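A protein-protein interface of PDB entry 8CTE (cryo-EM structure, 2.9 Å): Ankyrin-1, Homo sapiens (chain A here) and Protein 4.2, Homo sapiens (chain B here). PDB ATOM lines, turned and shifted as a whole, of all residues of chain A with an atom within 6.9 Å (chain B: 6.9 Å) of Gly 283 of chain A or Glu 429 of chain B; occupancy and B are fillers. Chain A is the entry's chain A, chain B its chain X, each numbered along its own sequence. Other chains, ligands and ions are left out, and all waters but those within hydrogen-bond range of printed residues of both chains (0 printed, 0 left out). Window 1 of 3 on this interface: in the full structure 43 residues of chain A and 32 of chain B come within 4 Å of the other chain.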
ATOM      1  N   HIS A 277      31.422   1.158  -6.086  1.00  0.00           N
ATOM      2  CA  HIS A 277      32.018   0.748  -7.355  1.00  0.00           C
ATOM      3  C   HIS A 277      31.503  -0.618  -7.792  1.00  0.00           C
ATOM      4  O   HIS A 277      31.188  -0.822  -8.971  1.00  0.00           O
ATOM      5  CB  HIS A 277      33.543   0.716  -7.244  1.00  0.00           C
ATOM      6  CG  HIS A 277      34.181   2.068  -7.169  1.00  0.00           C
ATOM      7  ND1 HIS A 277      34.529   2.660  -5.975  1.00  0.00           N
ATOM      8  CD2 HIS A 277      34.544   2.938  -8.139  1.00  0.00           C
ATOM      9  CE1 HIS A 277      35.075   3.838  -6.212  1.00  0.00           C
ATOM     10  NE2 HIS A 277      35.095   4.032  -7.519  1.00  0.00           N
ATOM     11  N   CYS A 278      31.421  -1.567  -6.855  1.00  0.00           N
ATOM     12  CA  CYS A 278      30.937  -2.904  -7.185  1.00  0.00           C
ATOM     13  C   CYS A 278      29.478  -2.873  -7.619  1.00  0.00           C
ATOM     14  O   CYS A 278      29.083  -3.588  -8.547  1.00  0.00           O
ATOM     15  CB  CYS A 278      31.123  -3.840  -5.990  1.00  0.00           C
ATOM     16  SG  CYS A 278      32.822  -3.959  -5.388  1.00  0.00           S
ATOM     17  N   ALA A 279      28.659  -2.057  -6.952  1.00  0.00           N
ATOM     18  CA  ALA A 279      27.258  -1.940  -7.339  1.00  0.00           C
ATOM     19  C   ALA A 279      27.111  -1.252  -8.692  1.00  0.00           C
ATOM     20  O   ALA A 279      26.235  -1.616  -9.486  1.00  0.00           O
ATOM     21  CB  ALA A 279      26.479  -1.183  -6.265  1.00  0.00           C
ATOM     22  N   ALA A 280      27.956  -0.258  -8.972  1.00  0.00           N
ATOM     23  CA  ALA A 280      27.821   0.509 -10.205  1.00  0.00           C
ATOM     24  C   ALA A 280      28.310  -0.278 -11.413  1.00  0.00           C
ATOM     25  O   ALA A 280      27.724  -0.182 -12.497  1.00  0.00           O
ATOM     26  CB  ALA A 280      28.577   1.831 -10.083  1.00  0.00           C
ATOM     27  N   ARG A 281      29.386  -1.052 -11.255  1.00  0.00           N
ATOM     28  CA  ARG A 281      29.920  -1.794 -12.391  1.00  0.00           C
ATOM     29  C   ARG A 281      29.020  -2.950 -12.804  1.00  0.00           C
ATOM     30  O   ARG A 281      29.150  -3.447 -13.929  1.00  0.00           O
ATOM     31  CB  ARG A 281      31.327  -2.308 -12.077  1.00  0.00           C
ATOM     32  CG  ARG A 281      31.385  -3.416 -11.043  1.00  0.00           C
ATOM     33  CD  ARG A 281      32.827  -3.781 -10.736  1.00  0.00           C
ATOM     34  NE  ARG A 281      33.601  -3.997 -11.953  1.00  0.00           N
ATOM     35  CZ  ARG A 281      34.896  -4.284 -11.978  1.00  0.00           C
ATOM     36  NH1 ARG A 281      35.598  -4.399 -10.864  1.00  0.00           N
ATOM     37  NH2 ARG A 281      35.499  -4.457 -13.150  1.00  0.00           N
ATOM     38  N   ASN A 282      28.114  -3.387 -11.932  1.00  0.00           N
ATOM     39  CA  ASN A 282      27.170  -4.446 -12.258  1.00  0.00           C
ATOM     40  C   ASN A 282      25.758  -3.933 -12.515  1.00  0.00           C
ATOM     41  O   ASN A 282      24.880  -4.732 -12.858  1.00  0.00           O
ATOM     42  CB  ASN A 282      27.141  -5.494 -11.140  1.00  0.00           C
ATOM     43  CG  ASN A 282      28.422  -6.305 -11.066  1.00  0.00           C
ATOM     44  OD1 ASN A 282      29.359  -5.944 -10.358  1.00  0.00           O
ATOM     45  ND2 ASN A 282      28.465  -7.412 -11.798  1.00  0.00           N
ATOM     46  N   GLY A 283      25.518  -2.633 -12.360  1.00  0.00           N
ATOM     47  CA  GLY A 283      24.228  -2.065 -12.695  1.00  0.00           C
ATOM     48  C   GLY A 283      23.139  -2.260 -11.669  1.00  0.00           C
ATOM     49  O   GLY A 283      21.958  -2.257 -12.030  1.00  0.00           O
ATOM     50  N   HIS A 284      23.491  -2.430 -10.399  1.00  0.00           N
ATOM     51  CA  HIS A 284      22.499  -2.600  -9.338  1.00  0.00           C
ATOM     52  C   HIS A 284      22.084  -1.216  -8.857  1.00  0.00           C
ATOM     53  O   HIS A 284      22.767  -0.597  -8.037  1.00  0.00           O
ATOM     54  CB  HIS A 284      23.064  -3.459  -8.213  1.00  0.00           C
ATOM     55  CG  HIS A 284      23.579  -4.786  -8.678  1.00  0.00           C
ATOM     56  ND1 HIS A 284      22.830  -5.641  -9.457  1.00  0.00           N
ATOM     57  CD2 HIS A 284      24.769  -5.400  -8.483  1.00  0.00           C
ATOM     58  CE1 HIS A 284      23.536  -6.725  -9.720  1.00  0.00           C
ATOM     59  NE2 HIS A 284      24.715  -6.605  -9.138  1.00  0.00           N
ATOM     60  N   VAL A 285      20.961  -0.725  -9.385  1.00  0.00           N
ATOM     61  CA  VAL A 285      20.519   0.634  -9.091  1.00  0.00           C
ATOM     62  C   VAL A 285      20.037   0.750  -7.650  1.00  0.00           C
ATOM     63  O   VAL A 285      20.340   1.731  -6.960  1.00  0.00           O
ATOM     64  CB  VAL A 285      19.429   1.059 -10.092  1.00  0.00           C
ATOM     65  CG1 VAL A 285      18.984   2.487  -9.826  1.00  0.00           C
ATOM     66  CG2 VAL A 285      19.940   0.914 -11.515  1.00  0.00           C
ATOM     67  N   ARG A 286      19.273  -0.239  -7.174  1.00  0.00           N
ATOM     68  CA  ARG A 286      18.731  -0.167  -5.819  1.00  0.00           C
ATOM     69  C   ARG A 286      19.839  -0.197  -4.773  1.00  0.00           C
ATOM     70  O   ARG A 286      19.796   0.557  -3.793  1.00  0.00           O
ATOM     71  CB  ARG A 286      17.745  -1.312  -5.585  1.00  0.00           C
ATOM     72  CG  ARG A 286      16.942  -1.181  -4.302  1.00  0.00           C
ATOM     73  CD  ARG A 286      15.975  -0.014  -4.379  1.00  0.00           C
ATOM     74  NE  ARG A 286      15.240   0.174  -3.134  1.00  0.00           N
ATOM     75  CZ  ARG A 286      15.528   1.095  -2.225  1.00  0.00           C
ATOM     76  NH1 ARG A 286      16.525   1.947  -2.396  1.00  0.00           N
ATOM     77  NH2 ARG A 286      14.794   1.166  -1.119  1.00  0.00           N
ATOM     78  N   SER A 288      22.963   0.748  -5.225  1.00  0.00           N
ATOM     79  CA  SER A 288      23.672   2.021  -5.314  1.00  0.00           C
ATOM     80  C   SER A 288      22.908   3.129  -4.600  1.00  0.00           C
ATOM     81  O   SER A 288      23.506   3.949  -3.895  1.00  0.00           O
ATOM     82  CB  SER A 288      23.908   2.390  -6.779  1.00  0.00           C
ATOM     83  OG  SER A 288      24.689   1.407  -7.435  1.00  0.00           O
ATOM     84  N   MET A 311      32.531   3.166 -13.787  1.00  0.00           N
ATOM     85  CA  MET A 311      32.153   1.756 -13.733  1.00  0.00           C
ATOM     86  C   MET A 311      30.782   1.525 -14.357  1.00  0.00           C
ATOM     87  O   MET A 311      30.580   0.542 -15.079  1.00  0.00           O
ATOM     88  CB  MET A 311      32.167   1.267 -12.285  1.00  0.00           C
ATOM     89  CG  MET A 311      33.523   1.328 -11.604  1.00  0.00           C
ATOM     90  SD  MET A 311      34.679   0.095 -12.229  1.00  0.00           S
ATOM     91  CE  MET A 311      36.051   0.319 -11.102  1.00  0.00           C
ATOM     92  N   ALA A 312      29.827   2.419 -14.084  1.00  0.00           N
ATOM     93  CA  ALA A 312      28.489   2.269 -14.648  1.00  0.00           C
ATOM     94  C   ALA A 312      28.497   2.452 -16.161  1.00  0.00           C
ATOM     95  O   ALA A 312      27.788   1.740 -16.881  1.00  0.00           O
ATOM     96  CB  ALA A 312      27.529   3.259 -13.988  1.00  0.00           C
ATOM     97  N   GLY A 315      29.924  -0.701 -18.061  1.00  0.00           N
ATOM     98  CA  GLY A 315      29.024  -1.828 -18.171  1.00  0.00           C
ATOM     99  C   GLY A 315      27.718  -1.580 -18.892  1.00  0.00           C
ATOM    100  O   GLY A 315      26.842  -2.450 -18.857  1.00  0.00           O
ATOM    101  N   ASP A 316      27.564  -0.422 -19.544  1.00  0.00           N
ATOM    102  CA  ASP A 316      26.326  -0.039 -20.235  1.00  0.00           C
ATOM    103  C   ASP A 316      25.130  -0.058 -19.285  1.00  0.00           C
ATOM    104  O   ASP A 316      24.032  -0.489 -19.644  1.00  0.00           O
ATOM    105  CB  ASP A 316      26.067  -0.926 -21.456  1.00  0.00           C
ATOM    106  CG  ASP A 316      25.121  -0.286 -22.456  1.00  0.00           C
ATOM    107  OD1 ASP A 316      24.742   0.887 -22.255  1.00  0.00           O
ATOM    108  OD2 ASP A 316      24.756  -0.958 -23.444  1.00  0.00           O
ATOM    109  N   HIS A 317      25.346   0.411 -18.057  1.00  0.00           N
ATOM    110  CA  HIS A 317      24.293   0.449 -17.042  1.00  0.00           C
ATOM    111  C   HIS A 317      23.660   1.837 -17.064  1.00  0.00           C
ATOM    112  O   HIS A 317      24.070   2.761 -16.359  1.00  0.00           O
ATOM    113  CB  HIS A 317      24.859   0.091 -15.676  1.00  0.00           C
ATOM    114  CG  HIS A 317      25.615  -1.202 -15.664  1.00  0.00           C
ATOM    115  ND1 HIS A 317      25.030  -2.407 -15.987  1.00  0.00           N
ATOM    116  CD2 HIS A 317      26.906  -1.479 -15.368  1.00  0.00           C
ATOM    117  CE1 HIS A 317      25.928  -3.370 -15.893  1.00  0.00           C
ATOM    118  NE2 HIS A 317      27.075  -2.834 -15.519  1.00  0.00           N
ATOM    119  N   LEU A 318      22.628   1.969 -17.900  1.00  0.00           N
ATOM    120  CA  LEU A 318      22.035   3.275 -18.171  1.00  0.00           C
ATOM    121  C   LEU A 318      21.340   3.847 -16.940  1.00  0.00           C
ATOM    122  O   LEU A 318      21.543   5.018 -16.589  1.00  0.00           O
ATOM    123  CB  LEU A 318      21.054   3.156 -19.336  1.00  0.00           C
ATOM    124  CG  LEU A 318      20.623   4.452 -20.013  1.00  0.00           C
ATOM    125  CD1 LEU A 318      21.851   5.206 -20.455  1.00  0.00           C
ATOM    126  CD2 LEU A 318      19.722   4.156 -21.196  1.00  0.00           C
ATOM    127  N   ASP A 319      20.516   3.037 -16.272  1.00  0.00           N
ATOM    128  CA  ASP A 319      19.789   3.531 -15.109  1.00  0.00           C
ATOM    129  C   ASP A 319      20.726   3.821 -13.945  1.00  0.00           C
ATOM    130  O   ASP A 319      20.463   4.733 -13.155  1.00  0.00           O
ATOM    131  CB  ASP A 319      18.713   2.527 -14.697  1.00  0.00           C
ATOM    132  CG  ASP A 319      17.649   3.148 -13.813  1.00  0.00           C
ATOM    133  OD1 ASP A 319      17.051   4.162 -14.229  1.00  0.00           O
ATOM    134  OD2 ASP A 319      17.405   2.622 -12.708  1.00  0.00           O
ATOM    135  N   CYS A 320      21.824   3.071 -13.828  1.00  0.00           N
ATOM    136  CA  CYS A 320      22.815   3.377 -12.802  1.00  0.00           C
ATOM    137  C   CYS A 320      23.493   4.714 -13.074  1.00  0.00           C
ATOM    138  O   CYS A 320      23.749   5.485 -12.142  1.00  0.00           O
ATOM    139  CB  CYS A 320      23.847   2.255 -12.713  1.00  0.00           C
ATOM    140  SG  CYS A 320      24.891   2.335 -11.244  1.00  0.00           S
ATOM    141  N   ARG A 322      22.058   7.194 -14.674  1.00  0.00           N
ATOM    142  CA  ARG A 322      21.031   8.177 -14.339  1.00  0.00           C
ATOM    143  C   ARG A 322      20.962   8.418 -12.836  1.00  0.00           C
ATOM    144  O   ARG A 322      20.866   9.564 -12.382  1.00  0.00           O
ATOM    145  CB  ARG A 322      19.668   7.719 -14.858  1.00  0.00           C
ATOM    146  CG  ARG A 322      19.529   7.662 -16.365  1.00  0.00           C
ATOM    147  CD  ARG A 322      18.056   7.652 -16.744  1.00  0.00           C
ATOM    148  NE  ARG A 322      17.832   7.354 -18.152  1.00  0.00           N
ATOM    149  CZ  ARG A 322      17.457   6.168 -18.614  1.00  0.00           C
ATOM    150  NH1 ARG A 322      17.270   5.139 -17.805  1.00  0.00           N
ATOM    151  NH2 ARG A 322      17.260   6.014 -19.920  1.00  0.00           N
ATOM    152  N   TYR B 158       9.510  -9.686  -9.625  1.00  0.00           N
ATOM    153  CA  TYR B 158       9.051 -10.471 -10.760  1.00  0.00           C
ATOM    154  C   TYR B 158       7.923 -11.438 -10.427  1.00  0.00           C
ATOM    155  O   TYR B 158       7.361 -12.034 -11.350  1.00  0.00           O
ATOM    156  CB  TYR B 158      10.228 -11.243 -11.364  1.00  0.00           C
ATOM    157  CG  TYR B 158      11.312 -10.345 -11.913  1.00  0.00           C
ATOM    158  CD1 TYR B 158      10.992  -9.214 -12.653  1.00  0.00           C
ATOM    159  CD2 TYR B 158      12.653 -10.616 -11.678  1.00  0.00           C
ATOM    160  CE1 TYR B 158      11.976  -8.386 -13.153  1.00  0.00           C
ATOM    161  CE2 TYR B 158      13.645  -9.791 -12.171  1.00  0.00           C
ATOM    162  CZ  TYR B 158      13.300  -8.678 -12.910  1.00  0.00           C
ATOM    163  OH  TYR B 158      14.280  -7.853 -13.407  1.00  0.00           O
ATOM    164  N   TYR B 167       6.187   0.146 -20.719  1.00  0.00           N
ATOM    165  CA  TYR B 167       6.810   1.294 -21.362  1.00  0.00           C
ATOM    166  C   TYR B 167       6.333   1.387 -22.805  1.00  0.00           C
ATOM    167  O   TYR B 167       6.484   0.435 -23.577  1.00  0.00           O
ATOM    168  CB  TYR B 167       8.332   1.188 -21.288  1.00  0.00           C
ATOM    169  CG  TYR B 167       8.847   1.236 -19.870  1.00  0.00           C
ATOM    170  CD1 TYR B 167       9.116   2.447 -19.249  1.00  0.00           C
ATOM    171  CD2 TYR B 167       9.043   0.068 -19.143  1.00  0.00           C
ATOM    172  CE1 TYR B 167       9.576   2.496 -17.949  1.00  0.00           C
ATOM    173  CE2 TYR B 167       9.503   0.108 -17.842  1.00  0.00           C
ATOM    174  CZ  TYR B 167       9.768   1.324 -17.251  1.00  0.00           C
ATOM    175  OH  TYR B 167      10.226   1.368 -15.955  1.00  0.00           O
ATOM    176  N   ARG B 287       8.280 -10.864 -16.570  1.00  0.00           N
ATOM    177  CA  ARG B 287       8.338  -9.419 -16.726  1.00  0.00           C
ATOM    178  C   ARG B 287       7.981  -9.063 -18.162  1.00  0.00           C
ATOM    179  O   ARG B 287       8.129  -9.873 -19.080  1.00  0.00           O
ATOM    180  CB  ARG B 287       9.721  -8.863 -16.364  1.00  0.00           C
ATOM    181  CG  ARG B 287      10.846  -9.352 -17.260  1.00  0.00           C
ATOM    182  CD  ARG B 287      12.182  -8.780 -16.816  1.00  0.00           C
ATOM    183  NE  ARG B 287      13.280  -9.217 -17.669  1.00  0.00           N
ATOM    184  CZ  ARG B 287      14.555  -8.918 -17.459  1.00  0.00           C
ATOM    185  NH1 ARG B 287      14.931  -8.186 -16.423  1.00  0.00           N
ATOM    186  NH2 ARG B 287      15.475  -9.364 -18.309  1.00  0.00           N
ATOM    187  N   ASN B 417      16.653   0.694 -27.280  1.00  0.00           N
ATOM    188  CA  ASN B 417      16.151   1.006 -25.940  1.00  0.00           C
ATOM    189  C   ASN B 417      15.215  -0.083 -25.421  1.00  0.00           C
ATOM    190  O   ASN B 417      14.092   0.180 -24.985  1.00  0.00           O
ATOM    191  CB  ASN B 417      15.466   2.374 -25.922  1.00  0.00           C
ATOM    192  CG  ASN B 417      16.419   3.506 -26.242  1.00  0.00           C
ATOM    193  OD1 ASN B 417      16.278   4.183 -27.258  1.00  0.00           O
ATOM    194  ND2 ASN B 417      17.399   3.717 -25.373  1.00  0.00           N
ATOM    195  N   ILE B 418      15.688  -1.326 -25.481  1.00  0.00           N
ATOM    196  CA  ILE B 418      14.943  -2.466 -24.961  1.00  0.00           C
ATOM    197  C   ILE B 418      14.817  -2.305 -23.452  1.00  0.00           C
ATOM    198  O   ILE B 418      15.811  -2.379 -22.722  1.00  0.00           O
ATOM    199  CB  ILE B 418      15.623  -3.793 -25.343  1.00  0.00           C
ATOM    200  CG1 ILE B 418      15.669  -3.934 -26.866  1.00  0.00           C
ATOM    201  CG2 ILE B 418      14.902  -4.966 -24.715  1.00  0.00           C
ATOM    202  CD1 ILE B 418      16.284  -5.225 -27.347  1.00  0.00           C
ATOM    203  N   SER B 419      13.595  -2.081 -22.977  1.00  0.00           N
ATOM    204  CA  SER B 419      13.362  -1.597 -21.626  1.00  0.00           C
ATOM    205  C   SER B 419      12.401  -2.501 -20.868  1.00  0.00           C
ATOM    206  O   SER B 419      11.545  -3.169 -21.456  1.00  0.00           O
ATOM    207  CB  SER B 419      12.807  -0.167 -21.646  1.00  0.00           C
ATOM    208  OG  SER B 419      13.698   0.720 -22.299  1.00  0.00           O
ATOM    209  N   THR B 420      12.561  -2.509 -19.547  1.00  0.00           N
ATOM    210  CA  THR B 420      11.659  -3.199 -18.637  1.00  0.00           C
ATOM    211  C   THR B 420      11.720  -2.482 -17.297  1.00  0.00           C
ATOM    212  O   THR B 420      12.621  -1.677 -17.047  1.00  0.00           O
ATOM    213  CB  THR B 420      12.023  -4.681 -18.484  1.00  0.00           C
ATOM    214  OG1 THR B 420      11.039  -5.335 -17.674  1.00  0.00           O
ATOM    215  CG2 THR B 420      13.389  -4.832 -17.833  1.00  0.00           C
ATOM    216  N   LYS B 421      10.742  -2.772 -16.444  1.00  0.00           N
ATOM    217  CA  LYS B 421      10.678  -2.127 -15.140  1.00  0.00           C
ATOM    218  C   LYS B 421      11.848  -2.566 -14.268  1.00  0.00           C
ATOM    219  O   LYS B 421      12.204  -3.746 -14.223  1.00  0.00           O
ATOM    220  CB  LYS B 421       9.353  -2.449 -14.449  1.00  0.00           C
ATOM    221  CG  LYS B 421       9.170  -1.746 -13.114  1.00  0.00           C
ATOM    222  CD  LYS B 421       7.854  -2.121 -12.458  1.00  0.00           C
ATOM    223  CE  LYS B 421       7.695  -1.426 -11.115  1.00  0.00           C
ATOM    224  NZ  LYS B 421       8.788  -1.785 -10.169  1.00  0.00           N
ATOM    225  N   GLY B 422      12.449  -1.602 -13.572  1.00  0.00           N
ATOM    226  CA  GLY B 422      13.576  -1.903 -12.716  1.00  0.00           C
ATOM    227  C   GLY B 422      13.174  -2.660 -11.466  1.00  0.00           C
ATOM    228  O   GLY B 422      12.000  -2.777 -11.115  1.00  0.00           O
ATOM    229  N   VAL B 423      14.185  -3.185 -10.780  1.00  0.00           N
ATOM    230  CA  VAL B 423      13.967  -3.981  -9.577  1.00  0.00           C
ATOM    231  C   VAL B 423      14.014  -3.065  -8.361  1.00  0.00           C
ATOM    232  O   VAL B 423      15.005  -2.363  -8.134  1.00  0.00           O
ATOM    233  CB  VAL B 423      15.007  -5.103  -9.461  1.00  0.00           C
ATOM    234  CG1 VAL B 423      14.832  -5.857  -8.154  1.00  0.00           C
ATOM    235  CG2 VAL B 423      14.896  -6.049 -10.646  1.00  0.00           C
ATOM    236  N   SER B 425      12.191  -0.384  -7.660  1.00  0.00           N
ATOM    237  CA  SER B 425      11.918   1.029  -7.888  1.00  0.00           C
ATOM    238  C   SER B 425      10.998   1.157  -9.095  1.00  0.00           C
ATOM    239  O   SER B 425      10.716   0.180  -9.795  1.00  0.00           O
ATOM    240  CB  SER B 425      13.215   1.819  -8.088  1.00  0.00           C
ATOM    241  OG  SER B 425      13.910   1.374  -9.240  1.00  0.00           O
ATOM    242  N   ARG B 427      11.908   3.023 -11.578  1.00  0.00           N
ATOM    243  CA  ARG B 427      12.812   3.462 -12.627  1.00  0.00           C
ATOM    244  C   ARG B 427      12.766   2.504 -13.813  1.00  0.00           C
ATOM    245  O   ARG B 427      12.234   1.395 -13.736  1.00  0.00           O
ATOM    246  CB  ARG B 427      14.239   3.563 -12.091  1.00  0.00           C
ATOM    247  CG  ARG B 427      14.354   4.361 -10.806  1.00  0.00           C
ATOM    248  CD  ARG B 427      15.788   4.404 -10.310  1.00  0.00           C
ATOM    249  NE  ARG B 427      16.675   5.046 -11.271  1.00  0.00           N
ATOM    250  CZ  ARG B 427      16.907   6.350 -11.322  1.00  0.00           C
ATOM    251  NH1 ARG B 427      16.331   7.187 -10.476  1.00  0.00           N
ATOM    252  NH2 ARG B 427      17.737   6.826 -12.245  1.00  0.00           N
ATOM    253  N   CYS B 428      13.339   2.953 -14.925  1.00  0.00           N
ATOM    254  CA  CYS B 428      13.379   2.179 -16.159  1.00  0.00           C
ATOM    255  C   CYS B 428      14.739   1.511 -16.301  1.00  0.00           C
ATOM    256  O   CYS B 428      15.776   2.174 -16.197  1.00  0.00           O
ATOM    257  CB  CYS B 428      13.098   3.072 -17.368  1.00  0.00           C
ATOM    258  SG  CYS B 428      13.076   2.202 -18.949  1.00  0.00           S
ATOM    259  N   GLU B 429      14.730   0.203 -16.536  1.00  0.00           N
ATOM    260  CA  GLU B 429      15.951  -0.573 -16.707  1.00  0.00           C
ATOM    261  C   GLU B 429      16.128  -0.917 -18.180  1.00  0.00           C
ATOM    262  O   GLU B 429      15.216  -1.462 -18.810  1.00  0.00           O
ATOM    263  CB  GLU B 429      15.911  -1.851 -15.867  1.00  0.00           C
ATOM    264  CG  GLU B 429      17.229  -2.609 -15.819  1.00  0.00           C
ATOM    265  CD  GLU B 429      18.271  -1.921 -14.955  1.00  0.00           C
ATOM    266  OE1 GLU B 429      17.890  -1.077 -14.117  1.00  0.00           O
ATOM    267  OE2 GLU B 429      19.471  -2.225 -15.114  1.00  0.00           O
ATOM    268  N   ASP B 430      17.299  -0.599 -18.723  1.00  0.00           N
ATOM    269  CA  ASP B 430      17.605  -0.868 -20.122  1.00  0.00           C
ATOM    270  C   ASP B 430      18.353  -2.192 -20.221  1.00  0.00           C
ATOM    271  O   ASP B 430      19.447  -2.338 -19.666  1.00  0.00           O
ATOM    272  CB  ASP B 430      18.428   0.272 -20.723  1.00  0.00           C
ATOM    273  CG  ASP B 430      18.335   0.326 -22.237  1.00  0.00           C
ATOM    274  OD1 ASP B 430      18.472  -0.732 -22.887  1.00  0.00           O
ATOM    275  OD2 ASP B 430      18.116   1.429 -22.777  1.00  0.00           O
ATOM    276  N   ILE B 431      17.764  -3.152 -20.931  1.00  0.00           N
ATOM    277  CA  ILE B 431      18.331  -4.486 -21.081  1.00  0.00           C
ATOM    278  C   ILE B 431      18.713  -4.780 -22.526  1.00  0.00           C
ATOM    279  O   ILE B 431      18.688  -5.943 -22.946  1.00  0.00           O
ATOM    280  CB  ILE B 431      17.377  -5.561 -20.535  1.00  0.00           C
ATOM    281  CG1 ILE B 431      16.004  -5.456 -21.202  1.00  0.00           C
ATOM    282  CG2 ILE B 431      17.243  -5.436 -19.026  1.00  0.00           C
ATOM    283  CD1 ILE B 431      15.039  -6.550 -20.797  1.00  0.00           C
ATOM    284  N   THR B 432      19.070  -3.752 -23.300  1.00  0.00           N
ATOM    285  CA  THR B 432      19.435  -3.963 -24.698  1.00  0.00           C
ATOM    286  C   THR B 432      20.715  -4.780 -24.824  1.00  0.00           C
ATOM    287  O   THR B 432      20.873  -5.560 -25.770  1.00  0.00           O
ATOM    288  CB  THR B 432      19.588  -2.616 -25.409  1.00  0.00           C
ATOM    289  OG1 THR B 432      18.458  -1.787 -25.112  1.00  0.00           O
ATOM    290  CG2 THR B 432      19.673  -2.813 -26.914  1.00  0.00           C
ATOM    291  N   GLN B 433      21.641  -4.620 -23.875  1.00  0.00           N
ATOM    292  CA  GLN B 433      22.891  -5.368 -23.911  1.00  0.00           C
ATOM    293  C   GLN B 433      22.691  -6.869 -23.743  1.00  0.00           C
ATOM    294  O   GLN B 433      23.573  -7.639 -24.137  1.00  0.00           O
ATOM    295  CB  GLN B 433      23.848  -4.852 -22.833  1.00  0.00           C
ATOM    296  CG  GLN B 433      23.290  -4.905 -21.423  1.00  0.00           C
ATOM    297  CD  GLN B 433      24.298  -4.446 -20.386  1.00  0.00           C
ATOM    298  OE1 GLN B 433      23.936  -4.090 -19.265  1.00  0.00           O
ATOM    299  NE2 GLN B 433      25.572  -4.454 -20.756  1.00  0.00           N
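Among the printed residues, pairs that only touch across the chains: Arg 322 of chain A with Arg 427 of chain B (3.4 Å), Leu 318 of chain A with Asp 430 of chain B (3.5 Å), Asp 316 of chain A with Gln 433 of chain B (3.6 Å), Arg 322 of chain A with Cys 428 of chain B (3.7 Å), Val 285 of chain A with Arg 427 of chain B (3.7 Å), Asp 319 of chain A with Glu 429 of chain B (3.7 Å), His 317 of chain A with Gln 433 of chain B (3.8 Å), Val 285 of chain A with Glu 429 of chain B (3.9 Å), Arg 286 of chain A with Val 423 of chain B (3.9 Å) and Gly 283 of chain A with Glu 429 of chain B (3.96 Å).
Of the 18 printed residues of chain B, 6 touch a printed residue of chain A. Of the 20 printed residues of chain A, 9 touch a printed residue of chain B. Hydrophobic or aromatic side chains of chain A that line the printed part of chain B: Val 285, His 317 and Leu 318. Among the printed residues, 13 pairs touch across the chains.
Of chain B, only Glu 429 (3.96 Å) comes within 4 Å of Gly 283 of chain A. Glu 429 of chain B touches three residues of chain A. Printed residues of chain A within 4 Å of Cys 428 of chain B: Asp 319 (3.1 Å) and Arg 322 (3.7 Å). Of the printed residues of chain A, Gln 433 of chain B touches Gly 315, Asp 316 and His 317. Printed residues of chain A within 4 Å of Arg 427 of chain B: Val 285, Asp 319 and Arg 322. The nearest printed residue of chain B that does not touch Gly 283 of chain A is Gln 433 of chain B (6.9 Å). The nearest printed residue of chain B that does not touch Val 285 of chain A is Ser 425 of chain B (5.2 Å).
O of Gly 315 of chain A is in hydrogen-bond range of NE2 of Gln 433 of chain B (3.0 Å). The guanidinium group (NE) of Arg 427 of chain B lies within salt-bridge range of the side-chain carboxylate (OD2) of Asp 319 of chain A (2.9 Å). O of Cys 428 of chain B sits close to OD1 of Asp 319 of chain A (3.1 Å).
The backbone carbonyl oxygen (O) of Arg 281 of chain A is in hydrogen-bond range of a ring nitrogen (NE2) of His 317 of chain A (2.7 Å). The backbone carbonyl oxygen of Ala 312 of chain A sits at hydrogen-bond distance from the backbone NH of His 317 of chain A, at 3.0 Å. O of Gly 315 of chain A lies close to NE2 of His 317 of chain A, at 3.4 Å. The side-chain carboxylate of Asp 319 of chain A lies within salt-bridge range of the guanidinium group of Arg 322 of chain A, at 3.7 Å. SG of Cys 428 of chain B sits close to OG of Ser 419 of chain B, 3.7 Å away. The side-chain carboxylate (OD1) of Asp 430 of chain B sits at hydrogen-bond distance from the side-chain hydroxyl (OG1) of Thr 432 of chain B (2.5 Å).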
